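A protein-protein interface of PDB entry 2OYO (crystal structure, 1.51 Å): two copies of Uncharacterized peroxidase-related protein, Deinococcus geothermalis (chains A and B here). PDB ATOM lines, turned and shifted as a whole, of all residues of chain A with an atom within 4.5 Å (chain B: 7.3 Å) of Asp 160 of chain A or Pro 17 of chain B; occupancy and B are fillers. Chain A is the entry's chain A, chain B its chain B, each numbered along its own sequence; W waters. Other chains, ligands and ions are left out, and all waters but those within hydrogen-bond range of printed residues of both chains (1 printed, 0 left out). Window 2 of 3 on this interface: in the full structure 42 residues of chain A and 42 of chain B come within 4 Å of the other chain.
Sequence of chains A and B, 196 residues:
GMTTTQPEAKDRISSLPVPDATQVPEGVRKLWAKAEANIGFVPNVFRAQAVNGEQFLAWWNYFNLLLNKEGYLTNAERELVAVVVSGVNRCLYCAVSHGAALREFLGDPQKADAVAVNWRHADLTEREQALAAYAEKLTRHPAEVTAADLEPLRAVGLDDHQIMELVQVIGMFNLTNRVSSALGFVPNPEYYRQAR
Printed residues of chain A that touch a printed residue of chain B: Arg 154, Asp 160, His 161, Ile 163 and Met 164.
Among the printed residues, 11 pairs touch across the chains.
Among the printed residues, no Asp or Glu carboxylate lies within 4 Å of a Lys or Arg side-chain nitrogen of the other chain.
Water W1 bridges NH2 of Arg 154 of chain A (2.7 Å) and O of Ser 15 of chain B (3.4 Å).
Of chain B, only Leu 16, Pro 17 and Val 51 come within 4 Å of Asp 160 of chain A.
Of chain A, only Asp 160 comes within 4 Å of Pro 17 of chain B.
Printed residues of chain B within 4 Å of Arg 154 of chain A: Leu 16.
Of the printed residues of chain A, Leu 183 of chain B touches Ile 163 and Met 164.
Printed residues of chain B within 4 Å of Ile 163 of chain A: Leu 183 (3.7 Å).
Printed residues of chain A within 4 Å of Asn 52 of chain B: His 161 (2.8 Å) and Met 164 (3.7 Å).
Of the printed residues of chain A, Val 51 of chain B touches Asp 160, His 161 and Met 164.
The nearest residue of chain B that does not touch Asp 160 of chain A is Asn 52 of chain B (4.8 Å).
The nearest printed residue of chain B that does not touch Arg 154 of chain A is Ser 15 of chain B (4.3 Å).
Among the printed residues, merely in contact across the chains: Arg 154 of chain A with Leu 16 of chain B (3.4 Å), Asp 160 of chain A with Leu 16 of chain B (3.6 Å), Asp 160 of chain A with Pro 17 of chain B (3.4 Å), Asp 160 of chain A with Val 51 of chain B (3.97 Å), Ile 163 of chain A with Leu 183 of chain B (3.7 Å), Met 164 of chain A with Gln 49 of chain B (3.8 Å), Met 164 of chain A with Val 51 of chain B (3.9 Å), Met 164 of chain A with Asn 52 of chain B (3.7 Å) and Met 164 of chain A with Leu 183 of chain B (3.8 Å).
The side-chain carboxylate (OD1) of Asp 160 of chain A is in salt-bridge range of the guanidinium group (NH1) of Arg 154 of chain A.
OD1 of Asp 159 of chain A lies within hydrogen-bond range of N of His 161 of chain A (3.1 Å).
The side-chain hydroxyl of Ser 14 of chain B lies within hydrogen-bond range of the backbone NH of Leu 16 of chain B (3.0 Å).
The backbone NH (N) of Ser 15 of chain B lies within hydrogen-bond range of the backbone carbonyl oxygen (O) of Leu 183 of chain B (2.7 Å).
No position is printed for both chains.
ND1 of His 161 of chain A sits close to O of Val 51 of chain B, 3.3 Å away.
A ring nitrogen (ND1) of His 161 of chain A is in hydrogen-bond range of the side-chain amide oxygen (OD1) of Asn 52 of chain B (2.8 Å).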
ATOM      1  N   ARG A 154      32.929   2.555  -4.588  1.00  0.00           N
ATOM      2  CA  ARG A 154      31.504   2.660  -4.351  1.00  0.00           C
ATOM      3  C   ARG A 154      31.169   3.894  -3.533  1.00  0.00           C
ATOM      4  O   ARG A 154      30.164   4.541  -3.806  1.00  0.00           O
ATOM      5  CB  ARG A 154      30.982   1.425  -3.660  1.00  0.00           C
ATOM      6  CG  ARG A 154      31.134   0.197  -4.468  1.00  0.00           C
ATOM      7  CD  ARG A 154      30.373  -0.956  -3.900  1.00  0.00           C
ATOM      8  NE  ARG A 154      30.715  -2.205  -4.566  1.00  0.00           N
ATOM      9  CZ  ARG A 154      30.155  -2.643  -5.697  1.00  0.00           C
ATOM     10  NH1 ARG A 154      29.218  -1.929  -6.345  1.00  0.00           N
ATOM     11  NH2 ARG A 154      30.544  -3.829  -6.187  1.00  0.00           N
ATOM     12  N   ASP A 159      28.996   2.527  -9.554  1.00  0.00           N
ATOM     13  CA  ASP A 159      28.213   1.291  -9.527  1.00  0.00           C
ATOM     14  C   ASP A 159      28.977   0.151 -10.223  1.00  0.00           C
ATOM     15  O   ASP A 159      30.119   0.321 -10.632  1.00  0.00           O
ATOM     16  CB  ASP A 159      26.828   1.518 -10.185  1.00  0.00           C
ATOM     17  CG  ASP A 159      26.900   1.808 -11.698  1.00  0.00           C
ATOM     18  OD1 ASP A 159      27.879   1.524 -12.413  1.00  0.00           O
ATOM     19  OD2 ASP A 159      25.897   2.318 -12.230  1.00  0.00           O
ATOM     20  N   ASP A 160      28.350  -1.014 -10.370  1.00  0.00           N
ATOM     21  CA  ASP A 160      29.062  -2.182 -10.851  1.00  0.00           C
ATOM     22  C   ASP A 160      29.535  -2.014 -12.277  1.00  0.00           C
ATOM     23  O   ASP A 160      30.619  -2.486 -12.658  1.00  0.00           O
ATOM     24  CB  ASP A 160      28.158  -3.405 -10.729  1.00  0.00           C
ATOM     25  CG  ASP A 160      27.836  -3.757  -9.268  1.00  0.00           C
ATOM     26  OD1 ASP A 160      28.736  -3.657  -8.415  1.00  0.00           O
ATOM     27  OD2 ASP A 160      26.687  -4.155  -8.972  1.00  0.00           O
ATOM     28  N   HIS A 161      28.737  -1.337 -13.111  1.00  0.00           N
ATOM     29  CA  HIS A 161      29.142  -1.117 -14.494  1.00  0.00           C
ATOM     30  C   HIS A 161      30.282  -0.146 -14.574  1.00  0.00           C
ATOM     31  O   HIS A 161      31.185  -0.294 -15.425  1.00  0.00           O
ATOM     32  CB  HIS A 161      28.010  -0.598 -15.331  1.00  0.00           C
ATOM     33  CG  HIS A 161      26.853  -1.531 -15.418  1.00  0.00           C
ATOM     34  ND1 HIS A 161      26.896  -2.688 -16.166  1.00  0.00           N
ATOM     35  CD2 HIS A 161      25.626  -1.486 -14.842  1.00  0.00           C
ATOM     36  CE1 HIS A 161      25.743  -3.326 -16.042  1.00  0.00           C
ATOM     37  NE2 HIS A 161      24.957  -2.620 -15.245  1.00  0.00           N
ATOM     38  N   GLN A 162      30.237   0.887 -13.733  1.00  0.00           N
ATOM     39  CA  GLN A 162      31.359   1.839 -13.715  1.00  0.00           C
ATOM     40  C   GLN A 162      32.673   1.169 -13.244  1.00  0.00           C
ATOM     41  O   GLN A 162      33.754   1.428 -13.817  1.00  0.00           O
ATOM     42  CB  GLN A 162      31.021   3.071 -12.872  1.00  0.00           C
ATOM     43  CG  GLN A 162      29.930   3.924 -13.489  1.00  0.00           C
ATOM     44  CD  GLN A 162      29.423   4.991 -12.567  1.00  0.00           C
ATOM     45  OE1 GLN A 162      28.799   4.722 -11.555  1.00  0.00           O
ATOM     46  NE2 GLN A 162      29.600   6.222 -12.974  1.00  0.00           N
ATOM     47  N   ILE A 163      32.582   0.314 -12.221  1.00  0.00           N
ATOM     48  CA  ILE A 163      33.765  -0.475 -11.765  1.00  0.00           C
ATOM     49  C   ILE A 163      34.298  -1.396 -12.865  1.00  0.00           C
ATOM     50  O   ILE A 163      35.488  -1.440 -13.110  1.00  0.00           O
ATOM     51  CB  ILE A 163      33.452  -1.194 -10.403  1.00  0.00           C
ATOM     52  CG1 ILE A 163      33.233  -0.151  -9.304  1.00  0.00           C
ATOM     53  CG2 ILE A 163      34.578  -2.182 -10.041  1.00  0.00           C
ATOM     54  CD1 ILE A 163      32.672  -0.679  -7.978  1.00  0.00           C
ATOM     55  N   MET A 164      33.414  -2.112 -13.545  1.00  0.00           N
ATOM     56  CA  MET A 164      33.766  -3.008 -14.646  1.00  0.00           C
ATOM     57  C   MET A 164      34.451  -2.235 -15.707  1.00  0.00           C
ATOM     58  O   MET A 164      35.417  -2.702 -16.250  1.00  0.00           O
ATOM     59  CB  MET A 164      32.511  -3.652 -15.221  1.00  0.00           C
ATOM     60  CG  MET A 164      32.762  -4.682 -16.270  1.00  0.00           C
ATOM     61  SD  MET A 164      33.436  -6.355 -15.614  1.00  0.00           S
ATOM     62  CE  MET A 164      35.143  -6.078 -16.359  1.00  0.00           C
ATOM     63  N   SER B  14      33.033 -13.999  -8.182  1.00  0.00           N
ATOM     64  CA  SER B  14      33.370 -12.625  -8.509  1.00  0.00           C
ATOM     65  C   SER B  14      33.020 -11.736  -7.343  1.00  0.00           C
ATOM     66  O   SER B  14      32.140 -12.069  -6.538  1.00  0.00           O
ATOM     67  CB  SER B  14      32.603 -12.176  -9.778  1.00  0.00           C
ATOM     68  OG  SER B  14      32.734 -10.797 -10.061  1.00  0.00           O
ATOM     69  N   SER B  15      33.732 -10.609  -7.243  1.00  0.00           N
ATOM     70  CA  SER B  15      33.410  -9.570  -6.294  1.00  0.00           C
ATOM     71  C   SER B  15      32.259  -8.692  -6.744  1.00  0.00           C
ATOM     72  O   SER B  15      31.722  -7.948  -5.940  1.00  0.00           O
ATOM     73  CB  SER B  15      34.640  -8.694  -6.040  1.00  0.00           C
ATOM     74  OG  SER B  15      35.701  -9.467  -5.490  1.00  0.00           O
ATOM     75  N   LEU B  16      31.899  -8.731  -8.031  1.00  0.00           N
ATOM     76  CA  LEU B  16      30.708  -8.044  -8.495  1.00  0.00           C
ATOM     77  C   LEU B  16      29.592  -9.063  -8.721  1.00  0.00           C
ATOM     78  O   LEU B  16      29.852 -10.251  -8.925  1.00  0.00           O
ATOM     79  CB  LEU B  16      30.972  -7.300  -9.825  1.00  0.00           C
ATOM     80  CG  LEU B  16      32.130  -6.293  -9.907  1.00  0.00           C
ATOM     81  CD1 LEU B  16      32.225  -5.696 -11.296  1.00  0.00           C
ATOM     82  CD2 LEU B  16      31.980  -5.214  -8.891  1.00  0.00           C
ATOM     83  N   PRO B  17      28.337  -8.594  -8.750  1.00  0.00           N
ATOM     84  CA  PRO B  17      27.242  -9.461  -9.208  1.00  0.00           C
ATOM     85  C   PRO B  17      27.545 -10.033 -10.568  1.00  0.00           C
ATOM     86  O   PRO B  17      28.180  -9.373 -11.420  1.00  0.00           O
ATOM     87  CB  PRO B  17      26.051  -8.523  -9.316  1.00  0.00           C
ATOM     88  CG  PRO B  17      26.320  -7.475  -8.296  1.00  0.00           C
ATOM     89  CD  PRO B  17      27.846  -7.274  -8.325  1.00  0.00           C
ATOM     90  N   VAL B  18      27.116 -11.276 -10.751  1.00  0.00           N
ATOM     91  CA  VAL B  18      27.287 -12.002 -11.992  1.00  0.00           C
ATOM     92  C   VAL B  18      25.923 -11.967 -12.748  1.00  0.00           C
ATOM     93  O   VAL B  18      24.877 -12.326 -12.178  1.00  0.00           O
ATOM     94  CB  VAL B  18      27.719 -13.447 -11.718  1.00  0.00           C
ATOM     95  CG1 VAL B  18      27.914 -14.222 -13.042  1.00  0.00           C
ATOM     96  CG2 VAL B  18      29.025 -13.477 -10.849  1.00  0.00           C
ATOM     97  N   PRO B  19      25.940 -11.518 -14.004  1.00  0.00           N
ATOM     98  CA  PRO B  19      24.700 -11.513 -14.770  1.00  0.00           C
ATOM     99  C   PRO B  19      24.278 -12.928 -15.156  1.00  0.00           C
ATOM    100  O   PRO B  19      25.109 -13.729 -15.525  1.00  0.00           O
ATOM    101  CB  PRO B  19      25.052 -10.704 -16.022  1.00  0.00           C
ATOM    102  CG  PRO B  19      26.557 -10.934 -16.231  1.00  0.00           C
ATOM    103  CD  PRO B  19      27.083 -10.975 -14.774  1.00  0.00           C
ATOM    104  N   ASP B  20      22.984 -13.195 -15.109  1.00  0.00           N
ATOM    105  CA  ASP B  20      22.448 -14.440 -15.657  1.00  0.00           C
ATOM    106  C   ASP B  20      22.128 -14.287 -17.151  1.00  0.00           C
ATOM    107  O   ASP B  20      22.427 -13.244 -17.754  1.00  0.00           O
ATOM    108  CB  ASP B  20      21.228 -14.917 -14.863  1.00  0.00           C
ATOM    109  CG  ASP B  20      20.049 -13.987 -14.975  1.00  0.00           C
ATOM    110  OD1 ASP B  20      19.869 -13.365 -16.033  1.00  0.00           O
ATOM    111  OD2 ASP B  20      19.307 -13.861 -13.977  1.00  0.00           O
ATOM    112  N   GLN B  23      20.472 -11.251 -18.622  1.00  0.00           N
ATOM    113  CA  GLN B  23      21.118  -9.963 -18.390  1.00  0.00           C
ATOM    114  C   GLN B  23      22.353  -9.773 -19.234  1.00  0.00           C
ATOM    115  O   GLN B  23      23.110  -8.826 -19.012  1.00  0.00           O
ATOM    116  CB  GLN B  23      21.507  -9.865 -16.928  1.00  0.00           C
ATOM    117  CG  GLN B  23      20.299  -9.819 -16.027  1.00  0.00           C
ATOM    118  CD  GLN B  23      20.606  -9.991 -14.568  1.00  0.00           C
ATOM    119  OE1 GLN B  23      21.487 -10.774 -14.160  1.00  0.00           O
ATOM    120  NE2 GLN B  23      19.830  -9.291 -13.745  1.00  0.00           N
ATOM    121  N   ARG B  47      31.041 -15.412 -17.490  1.00  0.00           N
ATOM    122  CA  ARG B  47      29.921 -14.924 -16.704  1.00  0.00           C
ATOM    123  C   ARG B  47      30.315 -13.663 -15.956  1.00  0.00           C
ATOM    124  O   ARG B  47      29.683 -12.608 -16.122  1.00  0.00           O
ATOM    125  CB  ARG B  47      29.402 -15.982 -15.740  1.00  0.00           C
ATOM    126  CG  ARG B  47      29.020 -17.304 -16.382  1.00  0.00           C
ATOM    127  CD  ARG B  47      28.475 -18.253 -15.352  1.00  0.00           C
ATOM    128  NE  ARG B  47      28.107 -19.552 -15.919  1.00  0.00           N
ATOM    129  CZ  ARG B  47      27.027 -19.785 -16.680  1.00  0.00           C
ATOM    130  NH1 ARG B  47      26.165 -18.832 -17.008  1.00  0.00           N
ATOM    131  NH2 ARG B  47      26.832 -21.012 -17.150  1.00  0.00           N
ATOM    132  N   ALA B  48      31.410 -13.740 -15.193  1.00  0.00           N
ATOM    133  CA  ALA B  48      31.754 -12.675 -14.279  1.00  0.00           C
ATOM    134  C   ALA B  48      32.152 -11.394 -15.016  1.00  0.00           C
ATOM    135  O   ALA B  48      31.852 -10.298 -14.572  1.00  0.00           O
ATOM    136  CB  ALA B  48      32.835 -13.155 -13.255  1.00  0.00           C
ATOM    137  N   GLN B  49      32.807 -11.547 -16.154  1.00  0.00           N
ATOM    138  CA  GLN B  49      33.254 -10.409 -16.918  1.00  0.00           C
ATOM    139  C   GLN B  49      32.232  -9.918 -17.944  1.00  0.00           C
ATOM    140  O   GLN B  49      32.470  -8.925 -18.650  1.00  0.00           O
ATOM    141  CB  GLN B  49      34.610 -10.736 -17.608  1.00  0.00           C
ATOM    142  CG  GLN B  49      35.405  -9.502 -17.995  1.00  0.00           C
ATOM    143  CD  GLN B  49      36.753  -9.795 -18.595  1.00  0.00           C
ATOM    144  OE1 GLN B  49      37.537 -10.644 -18.091  1.00  0.00           O
ATOM    145  NE2 GLN B  49      37.055  -9.077 -19.696  1.00  0.00           N
ATOM    146  N   ALA B  50      31.057 -10.549 -17.991  1.00  0.00           N
ATOM    147  CA  ALA B  50      29.986 -10.104 -18.880  1.00  0.00           C
ATOM    148  C   ALA B  50      29.106  -8.988 -18.285  1.00  0.00           C
ATOM    149  O   ALA B  50      28.103  -8.643 -18.861  1.00  0.00           O
ATOM    150  CB  ALA B  50      29.117 -11.321 -19.313  1.00  0.00           C
ATOM    151  N   VAL B  51      29.511  -8.425 -17.143  1.00  0.00           N
ATOM    152  CA  VAL B  51      28.812  -7.311 -16.523  1.00  0.00           C
ATOM    153  C   VAL B  51      28.554  -6.187 -17.537  1.00  0.00           C
ATOM    154  O   VAL B  51      27.443  -5.667 -17.586  1.00  0.00           O
ATOM    155  CB  VAL B  51      29.574  -6.774 -15.269  1.00  0.00           C
ATOM    156  CG1 VAL B  51      28.962  -5.430 -14.749  1.00  0.00           C
ATOM    157  CG2 VAL B  51      29.451  -7.838 -14.169  1.00  0.00           C
ATOM    158  N   ASN B  52      29.555  -5.808 -18.331  1.00  0.00           N
ATOM    159  CA  ASN B  52      29.348  -4.833 -19.422  1.00  0.00           C
ATOM    160  C   ASN B  52      29.406  -5.657 -20.687  1.00  0.00           C
ATOM    161  O   ASN B  52      30.476  -6.048 -21.138  1.00  0.00           O
ATOM    162  CB  ASN B  52      30.414  -3.701 -19.392  1.00  0.00           C
ATOM    163  CG  ASN B  52      30.282  -2.767 -18.157  1.00  0.00           C
ATOM    164  OD1 ASN B  52      29.418  -2.943 -17.312  1.00  0.00           O
ATOM    165  ND2 ASN B  52      31.168  -1.783 -18.064  1.00  0.00           N
ATOM    166  N   LEU B 183      38.691  -7.847  -9.550  1.00  0.00           N
ATOM    167  CA  LEU B 183      37.283  -8.231  -9.379  1.00  0.00           C
ATOM    168  C   LEU B 183      37.100  -9.626  -8.763  1.00  0.00           C
ATOM    169  O   LEU B 183      35.987 -10.138  -8.705  1.00  0.00           O
ATOM    170  CB  LEU B 183      36.550  -8.132 -10.715  1.00  0.00           C
ATOM    171  CG  LEU B 183      36.564  -6.722 -11.320  1.00  0.00           C
ATOM    172  CD1 LEU B 183      35.803  -6.756 -12.670  1.00  0.00           C
ATOM    173  CD2 LEU B 183      35.985  -5.632 -10.361  1.00  0.00           C
HETATM  174  O   HOH W   1      31.982  -5.043  -4.257  1.00  0.00           O
